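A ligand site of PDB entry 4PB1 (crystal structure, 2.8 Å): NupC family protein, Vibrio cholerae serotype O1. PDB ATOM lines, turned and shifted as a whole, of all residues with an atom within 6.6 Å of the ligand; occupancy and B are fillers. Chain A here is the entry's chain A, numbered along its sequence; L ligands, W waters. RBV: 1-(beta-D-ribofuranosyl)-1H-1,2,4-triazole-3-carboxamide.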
ATOM      1  N   VAL A 158       1.423  -8.059  18.150  1.00  0.00           N
ATOM      2  CA  VAL A 158       2.188  -7.144  17.299  1.00  0.00           C
ATOM      3  C   VAL A 158       2.054  -5.680  17.717  1.00  0.00           C
ATOM      4  O   VAL A 158       1.306  -5.347  18.631  1.00  0.00           O
ATOM      5  CB  VAL A 158       1.767  -7.276  15.822  1.00  0.00           C
ATOM      6  CG1 VAL A 158       1.966  -8.700  15.328  1.00  0.00           C
ATOM      7  CG2 VAL A 158       0.323  -6.837  15.634  1.00  0.00           C
ATOM      8  N   GLY A 159       2.795  -4.813  17.021  1.00  0.00           N
ATOM      9  CA  GLY A 159       2.877  -3.408  17.377  1.00  0.00           C
ATOM     10  C   GLY A 159       1.678  -2.563  17.005  1.00  0.00           C
ATOM     11  O   GLY A 159       0.761  -3.025  16.323  1.00  0.00           O
ATOM     12  N   GLN A 160       1.700  -1.305  17.424  1.00  0.00           N
ATOM     13  CA  GLN A 160       0.576  -0.388  17.246  1.00  0.00           C
ATOM     14  C   GLN A 160       0.313  -0.032  15.783  1.00  0.00           C
ATOM     15  O   GLN A 160      -0.785   0.426  15.446  1.00  0.00           O
ATOM     16  CB  GLN A 160       0.817   0.896  18.045  1.00  0.00           C
ATOM     17  CG  GLN A 160       2.091   1.634  17.690  1.00  0.00           C
ATOM     18  CD  GLN A 160       2.358   2.791  18.617  1.00  0.00           C
ATOM     19  OE1 GLN A 160       1.458   3.282  19.301  1.00  0.00           O
ATOM     20  NE2 GLN A 160       3.613   3.246  18.657  1.00  0.00           N
ATOM     21  N   THR A 161       1.298  -0.233  14.929  1.00  0.00           N
ATOM     22  CA  THR A 161       1.157   0.075  13.512  1.00  0.00           C
ATOM     23  C   THR A 161       0.864  -1.171  12.699  1.00  0.00           C
ATOM     24  O   THR A 161       0.273  -1.094  11.609  1.00  0.00           O
ATOM     25  CB  THR A 161       2.409   0.763  12.953  1.00  0.00           C
ATOM     26  OG1 THR A 161       3.582   0.059  13.384  1.00  0.00           O
ATOM     27  CG2 THR A 161       2.501   2.203  13.436  1.00  0.00           C
ATOM     28  N   GLU A 162       1.265  -2.325  13.219  1.00  0.00           N
ATOM     29  CA  GLU A 162       1.069  -3.592  12.513  1.00  0.00           C
ATOM     30  C   GLU A 162      -0.303  -4.188  12.809  1.00  0.00           C
ATOM     31  O   GLU A 162      -0.886  -4.876  11.972  1.00  0.00           O
ATOM     32  CB  GLU A 162       2.168  -4.588  12.890  1.00  0.00           C
ATOM     33  CG  GLU A 162       3.559  -4.210  12.409  1.00  0.00           C
ATOM     34  CD  GLU A 162       4.238  -3.149  13.265  1.00  0.00           C
ATOM     35  OE1 GLU A 162       3.691  -2.795  14.333  1.00  0.00           O
ATOM     36  OE2 GLU A 162       5.326  -2.667  12.874  1.00  0.00           O
ATOM     37  N   ILE A 190       2.518  -3.812  23.753  1.00  0.00           N
ATOM     38  CA  ILE A 190       3.803  -3.751  23.060  1.00  0.00           C
ATOM     39  C   ILE A 190       3.736  -4.590  21.793  1.00  0.00           C
ATOM     40  O   ILE A 190       2.708  -4.627  21.113  1.00  0.00           O
ATOM     41  CB  ILE A 190       4.972  -4.220  23.959  1.00  0.00           C
ATOM     42  CG1 ILE A 190       4.669  -5.580  24.596  1.00  0.00           C
ATOM     43  CG2 ILE A 190       5.242  -3.194  25.053  1.00  0.00           C
ATOM     44  CD1 ILE A 190       5.831  -6.133  25.397  1.00  0.00           C
ATOM     45  N   ALA A 191       4.843  -5.251  21.467  1.00  0.00           N
ATOM     46  CA  ALA A 191       4.881  -6.164  20.328  1.00  0.00           C
ATOM     47  C   ALA A 191       5.713  -7.392  20.675  1.00  0.00           C
ATOM     48  O   ALA A 191       6.529  -7.348  21.603  1.00  0.00           O
ATOM     49  CB  ALA A 191       5.442  -5.465  19.099  1.00  0.00           C
ATOM     50  N   VAL A 194       9.869  -6.906  20.703  1.00  0.00           N
ATOM     51  CA  VAL A 194      10.452  -6.233  21.870  1.00  0.00           C
ATOM     52  C   VAL A 194      10.166  -7.007  23.158  1.00  0.00           C
ATOM     53  O   VAL A 194      10.926  -6.903  24.123  1.00  0.00           O
ATOM     54  CB  VAL A 194       9.918  -4.794  22.023  1.00  0.00           C
ATOM     55  CG1 VAL A 194      10.507  -3.891  20.949  1.00  0.00           C
ATOM     56  CG2 VAL A 194       8.397  -4.769  21.978  1.00  0.00           C
ATOM     57  N   TYR A 198      12.966  -7.656  25.978  1.00  0.00           N
ATOM     58  CA  TYR A 198      12.871  -7.378  27.412  1.00  0.00           C
ATOM     59  C   TYR A 198      13.091  -8.655  28.222  1.00  0.00           C
ATOM     60  O   TYR A 198      13.699  -8.624  29.285  1.00  0.00           O
ATOM     61  CB  TYR A 198      11.500  -6.768  27.746  1.00  0.00           C
ATOM     62  CG  TYR A 198      11.207  -5.503  26.990  1.00  0.00           C
ATOM     63  CD1 TYR A 198      12.218  -4.611  26.666  1.00  0.00           C
ATOM     64  CD2 TYR A 198       9.910  -5.194  26.588  1.00  0.00           C
ATOM     65  CE1 TYR A 198      11.954  -3.448  25.973  1.00  0.00           C
ATOM     66  CE2 TYR A 198       9.633  -4.035  25.890  1.00  0.00           C
ATOM     67  CZ  TYR A 198      10.658  -3.164  25.586  1.00  0.00           C
ATOM     68  OH  TYR A 198      10.398  -2.005  24.885  1.00  0.00           O
ATOM     69  N   LEU A 265      13.899  -2.162  12.563  1.00  0.00           N
ATOM     70  CA  LEU A 265      13.479  -1.910  13.942  1.00  0.00           C
ATOM     71  C   LEU A 265      14.662  -2.026  14.903  1.00  0.00           C
ATOM     72  O   LEU A 265      14.813  -1.213  15.820  1.00  0.00           O
ATOM     73  CB  LEU A 265      12.374  -2.869  14.355  1.00  0.00           C
ATOM     74  CG  LEU A 265      11.826  -2.717  15.771  1.00  0.00           C
ATOM     75  CD1 LEU A 265      11.246  -1.324  15.975  1.00  0.00           C
ATOM     76  CD2 LEU A 265      10.798  -3.789  16.073  1.00  0.00           C
ATOM     77  N   VAL A 269      15.989   1.115  17.220  1.00  0.00           N
ATOM     78  CA  VAL A 269      16.003   0.972  18.675  1.00  0.00           C
ATOM     79  C   VAL A 269      17.410   1.183  19.227  1.00  0.00           C
ATOM     80  O   VAL A 269      17.604   1.875  20.226  1.00  0.00           O
ATOM     81  CB  VAL A 269      15.462  -0.400  19.107  1.00  0.00           C
ATOM     82  CG1 VAL A 269      15.820  -0.691  20.561  1.00  0.00           C
ATOM     83  CG2 VAL A 269      13.948  -0.466  18.913  1.00  0.00           C
ATOM     84  N   MET A 272      18.450   4.767  19.052  1.00  0.00           N
ATOM     85  CA  MET A 272      17.698   5.508  20.051  1.00  0.00           C
ATOM     86  C   MET A 272      18.303   5.324  21.441  1.00  0.00           C
ATOM     87  O   MET A 272      18.401   6.282  22.206  1.00  0.00           O
ATOM     88  CB  MET A 272      16.223   5.074  20.052  1.00  0.00           C
ATOM     89  CG  MET A 272      15.378   5.686  21.161  1.00  0.00           C
ATOM     90  SD  MET A 272      15.366   4.754  22.709  1.00  0.00           S
ATOM     91  CE  MET A 272      14.602   3.224  22.178  1.00  0.00           C
ATOM     92  N   ALA A 336       9.895   9.220  28.100  1.00  0.00           N
ATOM     93  CA  ALA A 336      10.677   8.728  26.963  1.00  0.00           C
ATOM     94  C   ALA A 336       9.982   7.542  26.298  1.00  0.00           C
ATOM     95  O   ALA A 336       9.012   7.718  25.553  1.00  0.00           O
ATOM     96  CB  ALA A 336      12.077   8.360  27.407  1.00  0.00           C
ATOM     97  N   ASN A 337      10.482   6.341  26.567  1.00  0.00           N
ATOM     98  CA  ASN A 337       9.816   5.128  26.128  1.00  0.00           C
ATOM     99  C   ASN A 337      10.135   3.958  27.063  1.00  0.00           C
ATOM    100  O   ASN A 337      11.047   4.040  27.883  1.00  0.00           O
ATOM    101  CB  ASN A 337      10.191   4.774  24.679  1.00  0.00           C
ATOM    102  CG  ASN A 337      11.679   4.564  24.490  1.00  0.00           C
ATOM    103  OD1 ASN A 337      12.223   3.536  24.878  1.00  0.00           O
ATOM    104  ND2 ASN A 337      12.342   5.538  23.868  1.00  0.00           N
ATOM    105  N   GLU A 338       9.378   2.872  26.936  1.00  0.00           N
ATOM    106  CA  GLU A 338       9.460   1.755  27.872  1.00  0.00           C
ATOM    107  C   GLU A 338      10.752   0.965  27.712  1.00  0.00           C
ATOM    108  O   GLU A 338      11.151   0.235  28.618  1.00  0.00           O
ATOM    109  CB  GLU A 338       8.251   0.828  27.692  1.00  0.00           C
ATOM    110  CG  GLU A 338       8.399  -0.215  26.588  1.00  0.00           C
ATOM    111  CD  GLU A 338       8.343   0.372  25.187  1.00  0.00           C
ATOM    112  OE1 GLU A 338       7.968   1.548  25.042  1.00  0.00           O
ATOM    113  OE2 GLU A 338       8.675  -0.359  24.227  1.00  0.00           O
ATOM    114  N   PHE A 339      11.407   1.098  26.567  1.00  0.00           N
ATOM    115  CA  PHE A 339      12.648   0.385  26.320  1.00  0.00           C
ATOM    116  C   PHE A 339      13.782   0.994  27.143  1.00  0.00           C
ATOM    117  O   PHE A 339      14.586   0.265  27.726  1.00  0.00           O
ATOM    118  CB  PHE A 339      12.986   0.407  24.827  1.00  0.00           C
ATOM    119  CG  PHE A 339      13.626  -0.858  24.338  1.00  0.00           C
ATOM    120  CD1 PHE A 339      13.119  -1.528  23.237  1.00  0.00           C
ATOM    121  CD2 PHE A 339      14.745  -1.378  24.966  1.00  0.00           C
ATOM    122  CE1 PHE A 339      13.703  -2.696  22.777  1.00  0.00           C
ATOM    123  CE2 PHE A 339      15.337  -2.537  24.518  1.00  0.00           C
ATOM    124  CZ  PHE A 339      14.819  -3.199  23.419  1.00  0.00           C
ATOM    125  N   VAL A 340      13.832   2.319  27.206  1.00  0.00           N
ATOM    126  CA  VAL A 340      14.815   3.027  28.014  1.00  0.00           C
ATOM    127  C   VAL A 340      14.577   2.764  29.498  1.00  0.00           C
ATOM    128  O   VAL A 340      15.525   2.647  30.273  1.00  0.00           O
ATOM    129  CB  VAL A 340      14.793   4.549  27.754  1.00  0.00           C
ATOM    130  CG1 VAL A 340      15.895   5.240  28.537  1.00  0.00           C
ATOM    131  CG2 VAL A 340      14.939   4.832  26.271  1.00  0.00           C
ATOM    132  N   GLY A 371       4.192  -1.272  27.941  1.00  0.00           N
ATOM    133  CA  GLY A 371       3.315  -0.603  26.992  1.00  0.00           C
ATOM    134  C   GLY A 371       4.018   0.449  26.154  1.00  0.00           C
ATOM    135  O   GLY A 371       5.034   1.014  26.574  1.00  0.00           O
ATOM    136  N   PHE A 372       3.475   0.730  24.974  1.00  0.00           N
ATOM    137  CA  PHE A 372       4.041   1.725  24.066  1.00  0.00           C
ATOM    138  C   PHE A 372       3.525   3.135  24.375  1.00  0.00           C
ATOM    139  O   PHE A 372       3.804   4.080  23.629  1.00  0.00           O
ATOM    140  CB  PHE A 372       3.736   1.368  22.605  1.00  0.00           C
ATOM    141  CG  PHE A 372       4.582   0.240  22.051  1.00  0.00           C
ATOM    142  CD1 PHE A 372       5.646  -0.275  22.774  1.00  0.00           C
ATOM    143  CD2 PHE A 372       4.327  -0.276  20.800  1.00  0.00           C
ATOM    144  CE1 PHE A 372       6.428  -1.297  22.264  1.00  0.00           C
ATOM    145  CE2 PHE A 372       5.100  -1.306  20.277  1.00  0.00           C
ATOM    146  CZ  PHE A 372       6.148  -1.808  21.010  1.00  0.00           C
ATOM    147  N   ALA A 373       2.778   3.265  25.458  1.00  0.00           N
ATOM    148  CA  ALA A 373       2.160   4.533  25.828  1.00  0.00           C
ATOM    149  C   ALA A 373       3.177   5.615  26.158  1.00  0.00           C
ATOM    150  O   ALA A 373       3.637   5.732  27.292  1.00  0.00           O
ATOM    151  CB  ALA A 373       1.209   4.338  27.009  1.00  0.00           C
ATOM    152  N   ASN A 374       3.531   6.402  25.145  1.00  0.00           N
ATOM    153  CA  ASN A 374       4.349   7.602  25.332  1.00  0.00           C
ATOM    154  C   ASN A 374       4.060   8.611  24.224  1.00  0.00           C
ATOM    155  O   ASN A 374       3.377   8.283  23.251  1.00  0.00           O
ATOM    156  CB  ASN A 374       5.842   7.243  25.360  1.00  0.00           C
ATOM    157  CG  ASN A 374       6.302   6.535  24.099  1.00  0.00           C
ATOM    158  OD1 ASN A 374       6.529   7.163  23.068  1.00  0.00           O
ATOM    159  ND2 ASN A 374       6.456   5.215  24.176  1.00  0.00           N
ATOM    160  N   SER A 376       6.016   9.969  22.019  1.00  0.00           N
ATOM    161  CA  SER A 376       6.701   9.734  20.755  1.00  0.00           C
ATOM    162  C   SER A 376       5.980   8.703  19.883  1.00  0.00           C
ATOM    163  O   SER A 376       6.224   8.622  18.679  1.00  0.00           O
ATOM    164  CB  SER A 376       8.142   9.269  21.009  1.00  0.00           C
ATOM    165  OG  SER A 376       8.918  10.344  21.513  1.00  0.00           O
ATOM    166  N   SER A 377       5.095   7.933  20.493  1.00  0.00           N
ATOM    167  CA  SER A 377       4.340   6.924  19.769  1.00  0.00           C
ATOM    168  C   SER A 377       3.209   7.553  18.954  1.00  0.00           C
ATOM    169  O   SER A 377       2.648   6.916  18.062  1.00  0.00           O
ATOM    170  CB  SER A 377       3.785   5.877  20.726  1.00  0.00           C
ATOM    171  OG  SER A 377       4.816   5.038  21.218  1.00  0.00           O
ATOM    172  N   ILE A 380       4.498   8.075  15.500  1.00  0.00           N
ATOM    173  CA  ILE A 380       4.507   6.772  14.840  1.00  0.00           C
ATOM    174  C   ILE A 380       3.090   6.386  14.423  1.00  0.00           C
ATOM    175  O   ILE A 380       2.892   5.767  13.380  1.00  0.00           O
ATOM    176  CB  ILE A 380       5.104   5.692  15.765  1.00  0.00           C
ATOM    177  CG1 ILE A 380       6.529   6.070  16.167  1.00  0.00           C
ATOM    178  CG2 ILE A 380       5.100   4.332  15.080  1.00  0.00           C
ATOM    179  CD1 ILE A 380       7.219   5.055  17.068  1.00  0.00           C
HETATM  180  N1  RBV L   1       8.324   0.593  18.869  1.00  0.00           N
HETATM  181  N2  RBV L   1       7.265   0.395  17.967  1.00  0.00           N
HETATM  182  C3  RBV L   1       7.357  -0.902  17.610  1.00  0.00           C
HETATM  183  N3  RBV L   1       6.746  -2.892  16.362  1.00  0.00           N
HETATM  184  O3  RBV L   1       5.488  -1.050  16.192  1.00  0.00           O
HETATM  185  N4  RBV L   1       8.414  -1.459  18.263  1.00  0.00           N
HETATM  186  C5  RBV L   1       9.005  -0.532  19.043  1.00  0.00           C
HETATM  187  C6  RBV L   1       6.463  -1.622  16.665  1.00  0.00           C
HETATM  188  C1' RBV L   1       8.460   1.961  19.432  1.00  0.00           C
HETATM  189  C2' RBV L   1       7.392   2.192  20.492  1.00  0.00           C
HETATM  190  O2' RBV L   1       6.885   3.525  20.400  1.00  0.00           O
HETATM  191  C3' RBV L   1       8.112   2.021  21.800  1.00  0.00           C
HETATM  192  O3' RBV L   1       7.594   2.912  22.793  1.00  0.00           O
HETATM  193  C4' RBV L   1       9.562   2.353  21.482  1.00  0.00           C
HETATM  194  O4' RBV L   1       9.721   2.069  20.088  1.00  0.00           O
HETATM  195  C5' RBV L   1      10.523   1.513  22.308  1.00  0.00           C
HETATM  196  O5' RBV L   1      10.172   0.129  22.173  1.00  0.00           O
HETATM  197  O   HOH W   1       8.142   5.973  21.391  1.00  0.00           O
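OE1 of Glu 162 sits close to O3 of the ligand, at 3.1 Å. Merely in contact with the ligand: Phe 372 (3.5 Å), Phe 339 (3.5 Å), Thr 161 (3.6 Å), Leu 265 (3.6 Å), Ile 380 (3.7 Å), Asn 337 (3.7 Å), Gly 159 (3.7 Å), Gln 160 (3.7 Å) and Ala 191 (3.98 Å). Within 4 Å of the ligand: Gly 159, Gln 160, Thr 161, Glu 162, Ala 191, Tyr 198, Leu 265, Asn 337, Glu 338, Phe 339, Phe 372, Asn 374, Ser 377 and Ile 380. The nearest printed residue that does not touch the ligand is Val 194 (4.1 Å).
An oxygen (O5') of the ligand is in hydrogen-bond range of the side-chain carboxylate of Glu 338. The side-chain hydroxyl (OG) of Ser 377 sits at hydrogen-bond distance from an oxygen (O2') of the ligand (2.7 Å). The side-chain amide nitrogen (ND2) of Asn 374 sits at hydrogen-bond distance from an oxygen (O3') of the ligand. OH of Tyr 198 sits at hydrogen-bond distance from O5' of the ligand (3.5 Å).
The side-chain hydroxyl (OH) of Tyr 198 lies within hydrogen-bond range of the side-chain carboxylate (OE2) of Glu 338 (2.5 Å). OD1 of Asn 374 lies within hydrogen-bond range of N of Ser 377 (3.0 Å). The side-chain hydroxyl of Ser 377 lies within hydrogen-bond range of the backbone carbonyl oxygen of Phe 372, 2.8 Å away. OG of Ser 377 lies within hydrogen-bond range of NE2 of Gln 160 (3.3 Å). The side-chain amide nitrogen of Asn 374 lies within hydrogen-bond range of the backbone carbonyl oxygen of Phe 372 (2.9 Å). OE1 of Glu 162 lies within hydrogen-bond range of OG1 of Thr 161 (3.0 Å). N of Gly 159 lies close to OE1 of Glu 162 (3.5 Å). The side-chain amide nitrogen (ND2) of Asn 337 is in hydrogen-bond range of the side-chain sulfur (SD) of Met 272, 3.3 Å away.
Water W1 lies within hydrogen-bond range of OD1 of Asn 374 (2.6 Å), O2' of the ligand (2.9 Å) and OG of Ser 377 (3.5 Å).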
